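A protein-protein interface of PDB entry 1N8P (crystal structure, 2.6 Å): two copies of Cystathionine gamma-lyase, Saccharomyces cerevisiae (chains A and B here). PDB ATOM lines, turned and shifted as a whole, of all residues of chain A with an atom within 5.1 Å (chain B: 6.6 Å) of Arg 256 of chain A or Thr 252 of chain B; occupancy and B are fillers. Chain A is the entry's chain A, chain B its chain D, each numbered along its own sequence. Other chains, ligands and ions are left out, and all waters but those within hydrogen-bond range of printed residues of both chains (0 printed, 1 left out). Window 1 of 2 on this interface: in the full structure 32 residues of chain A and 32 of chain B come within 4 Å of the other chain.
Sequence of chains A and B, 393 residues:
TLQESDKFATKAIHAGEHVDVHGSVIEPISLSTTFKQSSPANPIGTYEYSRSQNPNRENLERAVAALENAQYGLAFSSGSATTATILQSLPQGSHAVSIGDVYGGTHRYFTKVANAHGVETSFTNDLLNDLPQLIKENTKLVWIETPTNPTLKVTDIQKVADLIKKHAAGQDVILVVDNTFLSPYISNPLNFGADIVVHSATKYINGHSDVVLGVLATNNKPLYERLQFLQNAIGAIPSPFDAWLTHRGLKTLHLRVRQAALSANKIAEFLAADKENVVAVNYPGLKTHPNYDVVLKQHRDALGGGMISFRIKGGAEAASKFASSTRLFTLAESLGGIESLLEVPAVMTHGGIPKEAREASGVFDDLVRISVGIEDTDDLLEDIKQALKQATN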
ATOM      1  N   TYR A 204     -29.780 -33.779 -15.994  1.00  0.00           N
ATOM      2  CA  TYR A 204     -29.015 -33.784 -17.244  1.00  0.00           C
ATOM      3  C   TYR A 204     -29.293 -34.782 -18.340  1.00  0.00           C
ATOM      4  O   TYR A 204     -29.132 -34.433 -19.514  1.00  0.00           O
ATOM      5  CB  TYR A 204     -27.509 -33.856 -16.955  1.00  0.00           C
ATOM      6  CG  TYR A 204     -27.012 -32.754 -16.078  1.00  0.00           C
ATOM      7  CD1 TYR A 204     -27.180 -32.819 -14.697  1.00  0.00           C
ATOM      8  CD2 TYR A 204     -26.418 -31.615 -16.623  1.00  0.00           C
ATOM      9  CE1 TYR A 204     -26.758 -31.766 -13.867  1.00  0.00           C
ATOM     10  CE2 TYR A 204     -26.004 -30.552 -15.811  1.00  0.00           C
ATOM     11  CZ  TYR A 204     -26.173 -30.637 -14.434  1.00  0.00           C
ATOM     12  OH  TYR A 204     -25.757 -29.612 -13.621  1.00  0.00           O
ATOM     13  N   ILE A 205     -29.658 -36.015 -17.992  1.00  0.00           N
ATOM     14  CA  ILE A 205     -29.920 -37.056 -19.015  1.00  0.00           C
ATOM     15  C   ILE A 205     -31.100 -36.656 -19.937  1.00  0.00           C
ATOM     16  O   ILE A 205     -30.900 -36.410 -21.115  1.00  0.00           O
ATOM     17  CB  ILE A 205     -30.143 -38.475 -18.326  1.00  0.00           C
ATOM     18  CG1 ILE A 205     -28.814 -38.974 -17.745  1.00  0.00           C
ATOM     19  CG2 ILE A 205     -30.683 -39.506 -19.309  1.00  0.00           C
ATOM     20  CD1 ILE A 205     -28.968 -40.138 -16.801  1.00  0.00           C
ATOM     21  N   ASN A 206     -32.322 -36.589 -19.425  1.00  0.00           N
ATOM     22  CA  ASN A 206     -33.406 -36.168 -20.285  1.00  0.00           C
ATOM     23  C   ASN A 206     -33.079 -34.732 -20.640  1.00  0.00           C
ATOM     24  O   ASN A 206     -33.136 -34.331 -21.822  1.00  0.00           O
ATOM     25  CB  ASN A 206     -34.740 -36.211 -19.559  1.00  0.00           C
ATOM     26  CG  ASN A 206     -35.812 -35.466 -20.307  1.00  0.00           C
ATOM     27  OD1 ASN A 206     -35.903 -34.244 -20.242  1.00  0.00           O
ATOM     28  ND2 ASN A 206     -36.611 -36.191 -21.037  1.00  0.00           N
ATOM     29  N   GLY A 207     -32.763 -33.981 -19.572  1.00  0.00           N
ATOM     30  CA  GLY A 207     -32.360 -32.598 -19.646  1.00  0.00           C
ATOM     31  C   GLY A 207     -33.259 -31.513 -20.180  1.00  0.00           C
ATOM     32  O   GLY A 207     -32.784 -30.403 -20.440  1.00  0.00           O
ATOM     33  N   HIS A 208     -34.542 -31.793 -20.366  1.00  0.00           N
ATOM     34  CA  HIS A 208     -35.429 -30.765 -20.862  1.00  0.00           C
ATOM     35  C   HIS A 208     -36.503 -30.409 -19.838  1.00  0.00           C
ATOM     36  O   HIS A 208     -37.489 -29.737 -20.146  1.00  0.00           O
ATOM     37  CB  HIS A 208     -36.007 -31.220 -22.189  1.00  0.00           C
ATOM     38  CG  HIS A 208     -34.991 -31.254 -23.289  1.00  0.00           C
ATOM     39  ND1 HIS A 208     -34.813 -30.216 -24.170  1.00  0.00           N
ATOM     40  CD2 HIS A 208     -34.031 -32.155 -23.585  1.00  0.00           C
ATOM     41  CE1 HIS A 208     -33.789 -30.470 -24.962  1.00  0.00           C
ATOM     42  NE2 HIS A 208     -33.296 -31.642 -24.626  1.00  0.00           N
ATOM     43  N   GLY A 249     -33.802 -37.164 -25.046  1.00  0.00           N
ATOM     44  CA  GLY A 249     -33.045 -36.030 -24.573  1.00  0.00           C
ATOM     45  C   GLY A 249     -31.595 -36.461 -24.403  1.00  0.00           C
ATOM     46  O   GLY A 249     -30.639 -35.692 -24.614  1.00  0.00           O
ATOM     47  N   LEU A 250     -31.396 -37.711 -24.029  1.00  0.00           N
ATOM     48  CA  LEU A 250     -30.035 -38.209 -23.835  1.00  0.00           C
ATOM     49  C   LEU A 250     -29.144 -38.114 -25.101  1.00  0.00           C
ATOM     50  O   LEU A 250     -27.913 -38.117 -25.014  1.00  0.00           O
ATOM     51  CB  LEU A 250     -30.128 -39.645 -23.315  1.00  0.00           C
ATOM     52  CG  LEU A 250     -29.041 -40.711 -23.219  1.00  0.00           C
ATOM     53  CD1 LEU A 250     -29.684 -41.875 -22.502  1.00  0.00           C
ATOM     54  CD2 LEU A 250     -28.517 -41.137 -24.576  1.00  0.00           C
ATOM     55  N   THR A 252     -28.380 -35.674 -26.876  1.00  0.00           N
ATOM     56  CA  THR A 252     -27.629 -34.425 -26.972  1.00  0.00           C
ATOM     57  C   THR A 252     -26.876 -34.183 -25.667  1.00  0.00           C
ATOM     58  O   THR A 252     -26.220 -33.165 -25.508  1.00  0.00           O
ATOM     59  CB  THR A 252     -28.563 -33.217 -27.267  1.00  0.00           C
ATOM     60  OG1 THR A 252     -29.779 -33.362 -26.536  1.00  0.00           O
ATOM     61  CG2 THR A 252     -28.924 -33.138 -28.755  1.00  0.00           C
ATOM     62  N   LEU A 253     -26.958 -35.146 -24.748  1.00  0.00           N
ATOM     63  CA  LEU A 253     -26.301 -35.047 -23.457  1.00  0.00           C
ATOM     64  C   LEU A 253     -24.867 -34.586 -23.564  1.00  0.00           C
ATOM     65  O   LEU A 253     -24.414 -33.748 -22.769  1.00  0.00           O
ATOM     66  CB  LEU A 253     -26.304 -36.392 -22.743  1.00  0.00           C
ATOM     67  CG  LEU A 253     -25.552 -36.572 -21.417  1.00  0.00           C
ATOM     68  CD1 LEU A 253     -26.122 -35.690 -20.320  1.00  0.00           C
ATOM     69  CD2 LEU A 253     -25.685 -38.036 -21.005  1.00  0.00           C
ATOM     70  N   HIS A 254     -24.137 -35.146 -24.524  1.00  0.00           N
ATOM     71  CA  HIS A 254     -22.752 -34.750 -24.670  1.00  0.00           C
ATOM     72  C   HIS A 254     -22.625 -33.328 -25.187  1.00  0.00           C
ATOM     73  O   HIS A 254     -21.724 -32.603 -24.761  1.00  0.00           O
ATOM     74  CB  HIS A 254     -22.004 -35.730 -25.562  1.00  0.00           C
ATOM     75  CG  HIS A 254     -22.627 -35.913 -26.894  1.00  0.00           C
ATOM     76  ND1 HIS A 254     -22.124 -35.326 -28.030  1.00  0.00           N
ATOM     77  CD2 HIS A 254     -23.778 -36.523 -27.255  1.00  0.00           C
ATOM     78  CE1 HIS A 254     -22.950 -35.558 -29.035  1.00  0.00           C
ATOM     79  NE2 HIS A 254     -23.963 -36.283 -28.589  1.00  0.00           N
ATOM     80  N   LEU A 255     -23.495 -32.903 -26.095  1.00  0.00           N
ATOM     81  CA  LEU A 255     -23.391 -31.516 -26.556  1.00  0.00           C
ATOM     82  C   LEU A 255     -23.846 -30.536 -25.457  1.00  0.00           C
ATOM     83  O   LEU A 255     -23.191 -29.542 -25.193  1.00  0.00           O
ATOM     84  CB  LEU A 255     -24.207 -31.298 -27.822  1.00  0.00           C
ATOM     85  CG  LEU A 255     -23.726 -32.167 -28.988  1.00  0.00           C
ATOM     86  CD1 LEU A 255     -24.527 -31.843 -30.228  1.00  0.00           C
ATOM     87  CD2 LEU A 255     -22.243 -31.927 -29.235  1.00  0.00           C
ATOM     88  N   ARG A 256     -24.955 -30.825 -24.801  1.00  0.00           N
ATOM     89  CA  ARG A 256     -25.442 -29.950 -23.737  1.00  0.00           C
ATOM     90  C   ARG A 256     -24.457 -29.831 -22.582  1.00  0.00           C
ATOM     91  O   ARG A 256     -24.047 -28.745 -22.239  1.00  0.00           O
ATOM     92  CB  ARG A 256     -26.789 -30.439 -23.191  1.00  0.00           C
ATOM     93  CG  ARG A 256     -27.916 -30.309 -24.150  1.00  0.00           C
ATOM     94  CD  ARG A 256     -29.229 -30.668 -23.489  1.00  0.00           C
ATOM     95  NE  ARG A 256     -29.570 -32.080 -23.564  1.00  0.00           N
ATOM     96  CZ  ARG A 256     -29.299 -32.964 -22.616  1.00  0.00           C
ATOM     97  NH1 ARG A 256     -28.671 -32.576 -21.535  1.00  0.00           N
ATOM     98  NH2 ARG A 256     -29.711 -34.221 -22.726  1.00  0.00           N
ATOM     99  N   VAL A 257     -24.089 -30.949 -21.977  1.00  0.00           N
ATOM    100  CA  VAL A 257     -23.154 -30.964 -20.852  1.00  0.00           C
ATOM    101  C   VAL A 257     -21.791 -30.351 -21.147  1.00  0.00           C
ATOM    102  O   VAL A 257     -21.135 -29.806 -20.267  1.00  0.00           O
ATOM    103  CB  VAL A 257     -22.948 -32.377 -20.390  1.00  0.00           C
ATOM    104  CG1 VAL A 257     -21.832 -32.433 -19.404  1.00  0.00           C
ATOM    105  CG2 VAL A 257     -24.237 -32.898 -19.773  1.00  0.00           C
ATOM    106  N   ARG A 258     -21.366 -30.444 -22.397  1.00  0.00           N
ATOM    107  CA  ARG A 258     -20.080 -29.895 -22.814  1.00  0.00           C
ATOM    108  C   ARG A 258     -20.140 -28.372 -22.772  1.00  0.00           C
ATOM    109  O   ARG A 258     -19.186 -27.718 -22.385  1.00  0.00           O
ATOM    110  CB  ARG A 258     -19.747 -30.364 -24.254  1.00  0.00           C
ATOM    111  CG  ARG A 258     -18.327 -30.084 -24.741  1.00  0.00           C
ATOM    112  CD  ARG A 258     -17.353 -31.023 -24.083  1.00  0.00           C
ATOM    113  NE  ARG A 258     -15.964 -30.676 -24.360  1.00  0.00           N
ATOM    114  CZ  ARG A 258     -14.930 -31.179 -23.695  1.00  0.00           C
ATOM    115  NH1 ARG A 258     -15.125 -32.051 -22.714  1.00  0.00           N
ATOM    116  NH2 ARG A 258     -13.698 -30.802 -24.002  1.00  0.00           N
ATOM    117  N   GLN A 259     -21.276 -27.827 -23.185  1.00  0.00           N
ATOM    118  CA  GLN A 259     -21.490 -26.394 -23.240  1.00  0.00           C
ATOM    119  C   GLN A 259     -21.766 -25.800 -21.851  1.00  0.00           C
ATOM    120  O   GLN A 259     -21.193 -24.791 -21.459  1.00  0.00           O
ATOM    121  CB  GLN A 259     -22.664 -26.128 -24.159  1.00  0.00           C
ATOM    122  CG  GLN A 259     -22.999 -24.675 -24.331  1.00  0.00           C
ATOM    123  CD  GLN A 259     -21.956 -23.976 -25.088  1.00  0.00           C
ATOM    124  OE1 GLN A 259     -21.486 -24.476 -26.095  1.00  0.00           O
ATOM    125  NE2 GLN A 259     -21.569 -22.800 -24.627  1.00  0.00           N
ATOM    126  N   ALA A 260     -22.649 -26.440 -21.108  1.00  0.00           N
ATOM    127  CA  ALA A 260     -23.004 -25.969 -19.787  1.00  0.00           C
ATOM    128  C   ALA A 260     -21.751 -25.894 -18.921  1.00  0.00           C
ATOM    129  O   ALA A 260     -21.622 -25.029 -18.068  1.00  0.00           O
ATOM    130  CB  ALA A 260     -24.051 -26.904 -19.167  1.00  0.00           C
ATOM    131  N   ALA A 261     -20.815 -26.797 -19.165  1.00  0.00           N
ATOM    132  CA  ALA A 261     -19.582 -26.839 -18.394  1.00  0.00           C
ATOM    133  C   ALA A 261     -18.608 -25.692 -18.771  1.00  0.00           C
ATOM    134  O   ALA A 261     -18.129 -24.971 -17.889  1.00  0.00           O
ATOM    135  CB  ALA A 261     -18.917 -28.233 -18.558  1.00  0.00           C
ATOM    136  N   ILE A 338     -32.010 -27.387 -19.332  1.00  0.00           N
ATOM    137  CA  ILE A 338     -31.529 -26.809 -20.569  1.00  0.00           C
ATOM    138  C   ILE A 338     -31.448 -25.277 -20.416  1.00  0.00           C
ATOM    139  O   ILE A 338     -30.646 -24.587 -21.070  1.00  0.00           O
ATOM    140  CB  ILE A 338     -32.533 -27.270 -21.682  1.00  0.00           C
ATOM    141  CG1 ILE A 338     -31.972 -27.082 -23.051  1.00  0.00           C
ATOM    142  CG2 ILE A 338     -33.890 -26.556 -21.569  1.00  0.00           C
ATOM    143  CD1 ILE A 338     -32.931 -27.677 -24.036  1.00  0.00           C
ATOM    144  N   ILE A 374     -27.693 -23.704 -21.374  1.00  0.00           N
ATOM    145  CA  ILE A 374     -26.934 -23.662 -22.634  1.00  0.00           C
ATOM    146  C   ILE A 374     -27.124 -22.410 -23.503  1.00  0.00           C
ATOM    147  O   ILE A 374     -26.768 -22.404 -24.692  1.00  0.00           O
ATOM    148  CB  ILE A 374     -27.171 -24.951 -23.513  1.00  0.00           C
ATOM    149  CG1 ILE A 374     -28.633 -25.039 -23.992  1.00  0.00           C
ATOM    150  CG2 ILE A 374     -26.882 -26.188 -22.690  1.00  0.00           C
ATOM    151  CD1 ILE A 374     -28.892 -26.122 -25.045  1.00  0.00           C
ATOM    152  N   ALA B  12     -32.661 -19.190 -28.821  1.00  0.00           N
ATOM    153  CA  ALA B  12     -33.130 -20.566 -29.007  1.00  0.00           C
ATOM    154  C   ALA B  12     -33.820 -21.060 -27.763  1.00  0.00           C
ATOM    155  O   ALA B  12     -34.801 -21.767 -27.841  1.00  0.00           O
ATOM    156  CB  ALA B  12     -31.976 -21.486 -29.319  1.00  0.00           C
ATOM    157  N   ILE B  13     -33.274 -20.689 -26.613  1.00  0.00           N
ATOM    158  CA  ILE B  13     -33.787 -21.075 -25.298  1.00  0.00           C
ATOM    159  C   ILE B  13     -34.963 -20.276 -24.746  1.00  0.00           C
ATOM    160  O   ILE B  13     -35.803 -20.835 -24.048  1.00  0.00           O
ATOM    161  CB  ILE B  13     -32.661 -21.007 -24.222  1.00  0.00           C
ATOM    162  CG1 ILE B  13     -31.603 -22.079 -24.509  1.00  0.00           C
ATOM    163  CG2 ILE B  13     -33.231 -21.302 -22.842  1.00  0.00           C
ATOM    164  CD1 ILE B  13     -32.170 -23.468 -24.389  1.00  0.00           C
ATOM    165  N   TYR B 204     -33.766 -30.560 -39.199  1.00  0.00           N
ATOM    166  CA  TYR B 204     -32.916 -30.027 -38.150  1.00  0.00           C
ATOM    167  C   TYR B 204     -33.555 -29.217 -37.040  1.00  0.00           C
ATOM    168  O   TYR B 204     -33.067 -29.250 -35.908  1.00  0.00           O
ATOM    169  CB  TYR B 204     -31.847 -29.185 -38.780  1.00  0.00           C
ATOM    170  CG  TYR B 204     -31.080 -29.896 -39.862  1.00  0.00           C
ATOM    171  CD1 TYR B 204     -31.545 -29.902 -41.184  1.00  0.00           C
ATOM    172  CD2 TYR B 204     -29.835 -30.473 -39.590  1.00  0.00           C
ATOM    173  CE1 TYR B 204     -30.777 -30.446 -42.206  1.00  0.00           C
ATOM    174  CE2 TYR B 204     -29.065 -31.016 -40.605  1.00  0.00           C
ATOM    175  CZ  TYR B 204     -29.533 -30.995 -41.914  1.00  0.00           C
ATOM    176  OH  TYR B 204     -28.748 -31.485 -42.945  1.00  0.00           O
ATOM    177  N   ILE B 205     -34.615 -28.470 -37.341  1.00  0.00           N
ATOM    178  CA  ILE B 205     -35.250 -27.661 -36.288  1.00  0.00           C
ATOM    179  C   ILE B 205     -35.688 -28.608 -35.176  1.00  0.00           C
ATOM    180  O   ILE B 205     -35.190 -28.495 -34.049  1.00  0.00           O
ATOM    181  CB  ILE B 205     -36.449 -26.791 -36.824  1.00  0.00           C
ATOM    182  CG1 ILE B 205     -35.919 -25.674 -37.713  1.00  0.00           C
ATOM    183  CG2 ILE B 205     -37.177 -26.107 -35.685  1.00  0.00           C
ATOM    184  CD1 ILE B 205     -37.013 -24.839 -38.310  1.00  0.00           C
ATOM    185  N   ASN B 206     -36.596 -29.536 -35.482  1.00  0.00           N
ATOM    186  CA  ASN B 206     -37.039 -30.546 -34.501  1.00  0.00           C
ATOM    187  C   ASN B 206     -35.860 -31.496 -34.278  1.00  0.00           C
ATOM    188  O   ASN B 206     -35.638 -32.005 -33.185  1.00  0.00           O
ATOM    189  CB  ASN B 206     -38.200 -31.322 -35.057  1.00  0.00           C
ATOM    190  CG  ASN B 206     -38.485 -32.532 -34.273  1.00  0.00           C
ATOM    191  OD1 ASN B 206     -37.713 -33.459 -34.291  1.00  0.00           O
ATOM    192  ND2 ASN B 206     -39.595 -32.539 -33.565  1.00  0.00           N
ATOM    193  N   HIS B 208     -35.007 -34.488 -34.546  1.00  0.00           N
ATOM    194  CA  HIS B 208     -35.046 -35.876 -34.127  1.00  0.00           C
ATOM    195  C   HIS B 208     -35.865 -36.737 -35.060  1.00  0.00           C
ATOM    196  O   HIS B 208     -36.109 -37.900 -34.792  1.00  0.00           O
ATOM    197  CB  HIS B 208     -35.547 -35.966 -32.680  1.00  0.00           C
ATOM    198  CG  HIS B 208     -34.571 -35.399 -31.690  1.00  0.00           C
ATOM    199  ND1 HIS B 208     -33.789 -36.188 -30.876  1.00  0.00           N
ATOM    200  CD2 HIS B 208     -34.208 -34.114 -31.439  1.00  0.00           C
ATOM    201  CE1 HIS B 208     -32.981 -35.412 -30.168  1.00  0.00           C
ATOM    202  NE2 HIS B 208     -33.214 -34.150 -30.490  1.00  0.00           N
ATOM    203  N   HIS B 247     -40.641 -27.557 -30.787  1.00  0.00           N
ATOM    204  CA  HIS B 247     -40.118 -26.430 -30.021  1.00  0.00           C
ATOM    205  C   HIS B 247     -39.090 -26.983 -29.038  1.00  0.00           C
ATOM    206  O   HIS B 247     -38.050 -26.388 -28.789  1.00  0.00           O
ATOM    207  CB  HIS B 247     -41.245 -25.751 -29.255  1.00  0.00           C
ATOM    208  CG  HIS B 247     -40.943 -24.342 -28.843  1.00  0.00           C
ATOM    209  ND1 HIS B 247     -39.668 -23.825 -28.813  1.00  0.00           N
ATOM    210  CD2 HIS B 247     -41.759 -23.342 -28.438  1.00  0.00           C
ATOM    211  CE1 HIS B 247     -39.710 -22.569 -28.412  1.00  0.00           C
ATOM    212  NE2 HIS B 247     -40.968 -22.251 -28.174  1.00  0.00           N
ATOM    213  N   ARG B 248     -39.389 -28.134 -28.462  1.00  0.00           N
ATOM    214  CA  ARG B 248     -38.451 -28.758 -27.558  1.00  0.00           C
ATOM    215  C   ARG B 248     -37.166 -29.079 -28.284  1.00  0.00           C
ATOM    216  O   ARG B 248     -36.088 -28.916 -27.719  1.00  0.00           O
ATOM    217  CB  ARG B 248     -39.013 -30.048 -27.059  1.00  0.00           C
ATOM    218  CG  ARG B 248     -38.060 -30.844 -26.225  1.00  0.00           C
ATOM    219  CD  ARG B 248     -38.708 -32.199 -26.026  1.00  0.00           C
ATOM    220  NE  ARG B 248     -38.453 -32.812 -24.750  1.00  0.00           N
ATOM    221  CZ  ARG B 248     -37.576 -33.776 -24.584  1.00  0.00           C
ATOM    222  NH1 ARG B 248     -36.902 -34.201 -25.638  1.00  0.00           N
ATOM    223  NH2 ARG B 248     -37.374 -34.295 -23.382  1.00  0.00           N
ATOM    224  N   GLY B 249     -37.304 -29.562 -29.532  1.00  0.00           N
ATOM    225  CA  GLY B 249     -36.169 -29.927 -30.370  1.00  0.00           C
ATOM    226  C   GLY B 249     -35.319 -28.768 -30.813  1.00  0.00           C
ATOM    227  O   GLY B 249     -34.095 -28.850 -30.884  1.00  0.00           O
ATOM    228  N   LEU B 250     -35.979 -27.666 -31.100  1.00  0.00           N
ATOM    229  CA  LEU B 250     -35.331 -26.442 -31.536  1.00  0.00           C
ATOM    230  C   LEU B 250     -34.288 -25.880 -30.550  1.00  0.00           C
ATOM    231  O   LEU B 250     -33.341 -25.213 -30.958  1.00  0.00           O
ATOM    232  CB  LEU B 250     -36.443 -25.421 -31.815  1.00  0.00           C
ATOM    233  CG  LEU B 250     -36.221 -23.915 -31.985  1.00  0.00           C
ATOM    234  CD1 LEU B 250     -37.311 -23.356 -32.898  1.00  0.00           C
ATOM    235  CD2 LEU B 250     -36.254 -23.219 -30.625  1.00  0.00           C
ATOM    236  N   LYS B 251     -34.449 -26.164 -29.261  1.00  0.00           N
ATOM    237  CA  LYS B 251     -33.552 -25.656 -28.206  1.00  0.00           C
ATOM    238  C   LYS B 251     -32.101 -26.117 -28.203  1.00  0.00           C
ATOM    239  O   LYS B 251     -31.284 -25.563 -27.462  1.00  0.00           O
ATOM    240  CB  LYS B 251     -34.156 -25.954 -26.821  1.00  0.00           C
ATOM    241  CG  LYS B 251     -35.496 -25.274 -26.591  1.00  0.00           C
ATOM    242  CD  LYS B 251     -36.011 -25.562 -25.227  1.00  0.00           C
ATOM    243  CE  LYS B 251     -37.308 -24.829 -24.962  1.00  0.00           C
ATOM    244  NZ  LYS B 251     -37.053 -23.599 -24.167  1.00  0.00           N
ATOM    245  N   THR B 252     -31.778 -27.138 -28.993  1.00  0.00           N
ATOM    246  CA  THR B 252     -30.414 -27.651 -29.045  1.00  0.00           C
ATOM    247  C   THR B 252     -29.933 -27.525 -30.455  1.00  0.00           C
ATOM    248  O   THR B 252     -28.914 -28.094 -30.804  1.00  0.00           O
ATOM    249  CB  THR B 252     -30.356 -29.126 -28.657  1.00  0.00           C
ATOM    250  OG1 THR B 252     -31.579 -29.742 -29.031  1.00  0.00           O
ATOM    251  CG2 THR B 252     -30.220 -29.311 -27.163  1.00  0.00           C
ATOM    252  N   LEU B 253     -30.681 -26.769 -31.263  1.00  0.00           N
ATOM    253  CA  LEU B 253     -30.377 -26.546 -32.678  1.00  0.00           C
ATOM    254  C   LEU B 253     -29.014 -25.938 -32.947  1.00  0.00           C
ATOM    255  O   LEU B 253     -28.340 -26.351 -33.878  1.00  0.00           O
ATOM    256  CB  LEU B 253     -31.456 -25.673 -33.300  1.00  0.00           C
ATOM    257  CG  LEU B 253     -31.303 -25.281 -34.757  1.00  0.00           C
ATOM    258  CD1 LEU B 253     -31.208 -26.493 -35.622  1.00  0.00           C
ATOM    259  CD2 LEU B 253     -32.489 -24.457 -35.153  1.00  0.00           C
ATOM    260  N   HIS B 254     -28.621 -24.944 -32.153  1.00  0.00           N
ATOM    261  CA  HIS B 254     -27.316 -24.313 -32.315  1.00  0.00           C
ATOM    262  C   HIS B 254     -26.209 -25.317 -31.941  1.00  0.00           C
ATOM    263  O   HIS B 254     -25.180 -25.397 -32.575  1.00  0.00           O
ATOM    264  CB  HIS B 254     -27.233 -23.022 -31.466  1.00  0.00           C
ATOM    265  CG  HIS B 254     -27.556 -23.205 -30.014  1.00  0.00           C
ATOM    266  ND1 HIS B 254     -26.583 -23.300 -29.038  1.00  0.00           N
ATOM    267  CD2 HIS B 254     -28.744 -23.307 -29.367  1.00  0.00           C
ATOM    268  CE1 HIS B 254     -27.154 -23.449 -27.854  1.00  0.00           C
ATOM    269  NE2 HIS B 254     -28.466 -23.456 -28.026  1.00  0.00           N
ATOM    270  N   LEU B 255     -26.434 -26.098 -30.904  1.00  0.00           N
ATOM    271  CA  LEU B 255     -25.477 -27.090 -30.527  1.00  0.00           C
ATOM    272  C   LEU B 255     -25.355 -28.160 -31.642  1.00  0.00           C
ATOM    273  O   LEU B 255     -24.305 -28.299 -32.258  1.00  0.00           O
ATOM    274  CB  LEU B 255     -25.916 -27.677 -29.194  1.00  0.00           C
ATOM    275  CG  LEU B 255     -25.637 -26.670 -28.069  1.00  0.00           C
ATOM    276  CD1 LEU B 255     -25.736 -27.381 -26.707  1.00  0.00           C
ATOM    277  CD2 LEU B 255     -24.216 -26.055 -28.272  1.00  0.00           C
ATOM    278  N   ARG B 256     -26.448 -28.866 -31.915  1.00  0.00           N
ATOM    279  CA  ARG B 256     -26.543 -29.900 -32.956  1.00  0.00           C
ATOM    280  C   ARG B 256     -26.047 -29.565 -34.364  1.00  0.00           C
ATOM    281  O   ARG B 256     -25.497 -30.428 -35.025  1.00  0.00           O
ATOM    282  CB  ARG B 256     -27.986 -30.358 -33.121  1.00  0.00           C
ATOM    283  CG  ARG B 256     -28.612 -30.864 -31.864  1.00  0.00           C
ATOM    284  CD  ARG B 256     -29.829 -31.719 -32.184  1.00  0.00           C
ATOM    285  NE  ARG B 256     -31.071 -30.975 -32.090  1.00  0.00           N
ATOM    286  CZ  ARG B 256     -31.534 -30.189 -33.037  1.00  0.00           C
ATOM    287  NH1 ARG B 256     -30.861 -30.043 -34.152  1.00  0.00           N
ATOM    288  NH2 ARG B 256     -32.684 -29.572 -32.874  1.00  0.00           N
ATOM    289  N   VAL B 257     -26.272 -28.342 -34.842  1.00  0.00           N
ATOM    290  CA  VAL B 257     -25.841 -27.952 -36.182  1.00  0.00           C
ATOM    291  C   VAL B 257     -24.387 -27.581 -36.227  1.00  0.00           C
ATOM    292  O   VAL B 257     -23.707 -27.822 -37.224  1.00  0.00           O
ATOM    293  CB  VAL B 257     -26.650 -26.788 -36.692  1.00  0.00           C
ATOM    294  CG1 VAL B 257     -25.885 -26.071 -37.779  1.00  0.00           C
ATOM    295  CG2 VAL B 257     -28.006 -27.298 -37.236  1.00  0.00           C
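Thr 252 of chain A touches Arg 256 of chain B, and with the chains exchanged Arg 256 of chain A touches Thr 252 of chain B.
Leu 255 of chain A touches its own counterpart, Leu 255 of chain B.
Leu 255 of chain A touches Arg 256 of chain B, and with the chains exchanged Arg 256 of chain A touches Leu 255 of chain B.
12 positions are printed for both chains.
Of the 14 pairs that touch across the chains among the printed residues, 5 have their exchanged pair printed and touching as well.
NH2 of Arg 256 of chain B sits at hydrogen-bond distance from O of Ile 205 of chain B.
OG1 of Thr 252 of chain B lies within hydrogen-bond range of O of Gly 249 of chain B.
N of Ile 374 of chain A lies within hydrogen-bond range of O of Ile 338 of chain A (3.1 Å).
The backbone carbonyl oxygen of Ile 13 of chain B lies within hydrogen-bond range of the side-chain amino group of Lys 251 of chain B (3.0 Å).
N of Ile 338 of chain A is in hydrogen-bond range of O of Gly 207 of chain A, at 3.3 Å.
OD1 of Asn 206 of chain A is in hydrogen-bond range of N of His 208 of chain A, at 2.8 Å.
The side-chain amide nitrogen (ND2) of Asn 206 of chain A lies close to the guanidinium group (NH2) of Arg 248 of chain B.
Of the 17 printed residues of chain B, 7 touch a printed residue of chain A.
Printed residues of chain B that touch a printed residue of chain A: Ile 13, Arg 248, Lys 251, Thr 252, His 254, Leu 255 and Arg 256.
Hydrophobic or aromatic side chains of chain B within 4 Å of the printed part of chain A: Ile 13, His 254 and Leu 255.
Printed residues of chain A that touch a printed residue of chain B: Asn 206, His 208, Thr 252, Leu 255, Arg 256, Gln 259, Ile 338 and Ile 374.
Hydrophobic or aromatic side chains of chain A within 4 Å of the printed part of chain B: His 208, Leu 255, Ile 338 and Ile 374.
Among the printed residues, 14 pairs touch across the chains.
His 208 of chain A touches Arg 248 of chain B (CB to NH2, 3.6 Å).
Thr 252 of chain A touches Arg 256 of chain B (CG2 to CD, 3.8 Å).
CD1 of Leu 255 of chain B touches O of Leu 255 of chain A (3.7 Å).
CD1 of Leu 255 of chain A touches CA of Arg 256 of chain B (3.9 Å).
CG of Arg 256 of chain A touches CG2 of Thr 252 of chain B (3.9 Å).
CD1 of Ile 338 of chain A touches CB of Lys 251 of chain B, at 3.5 Å.
Ile 374 of chain A touches Ile 13 of chain B.
Ile 374 of chain A touches Lys 251 of chain B.
O of Ile 374 of chain A touches CE1 of His 254 of chain B, at 3.4 Å.
CD1 of Leu 255 of chain B touches CD1 of Ile 374 of chain A, at 3.8 Å.
Printed residues of chain B within 4 Å of Thr 252 of chain A: Arg 256.
Of the printed residues of chain B, Leu 255 of chain A touches Leu 255 and Arg 256.
Of chain B, only Thr 252 and Leu 255 come within 4 Å of Arg 256 of chain A.
Of the printed residues of chain A, Lys 251 of chain B touches Ile 338 and Ile 374.
Printed residues of chain A within 4 Å of Leu 255 of chain B: Leu 255, Arg 256, Gln 259 and Ile 374.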
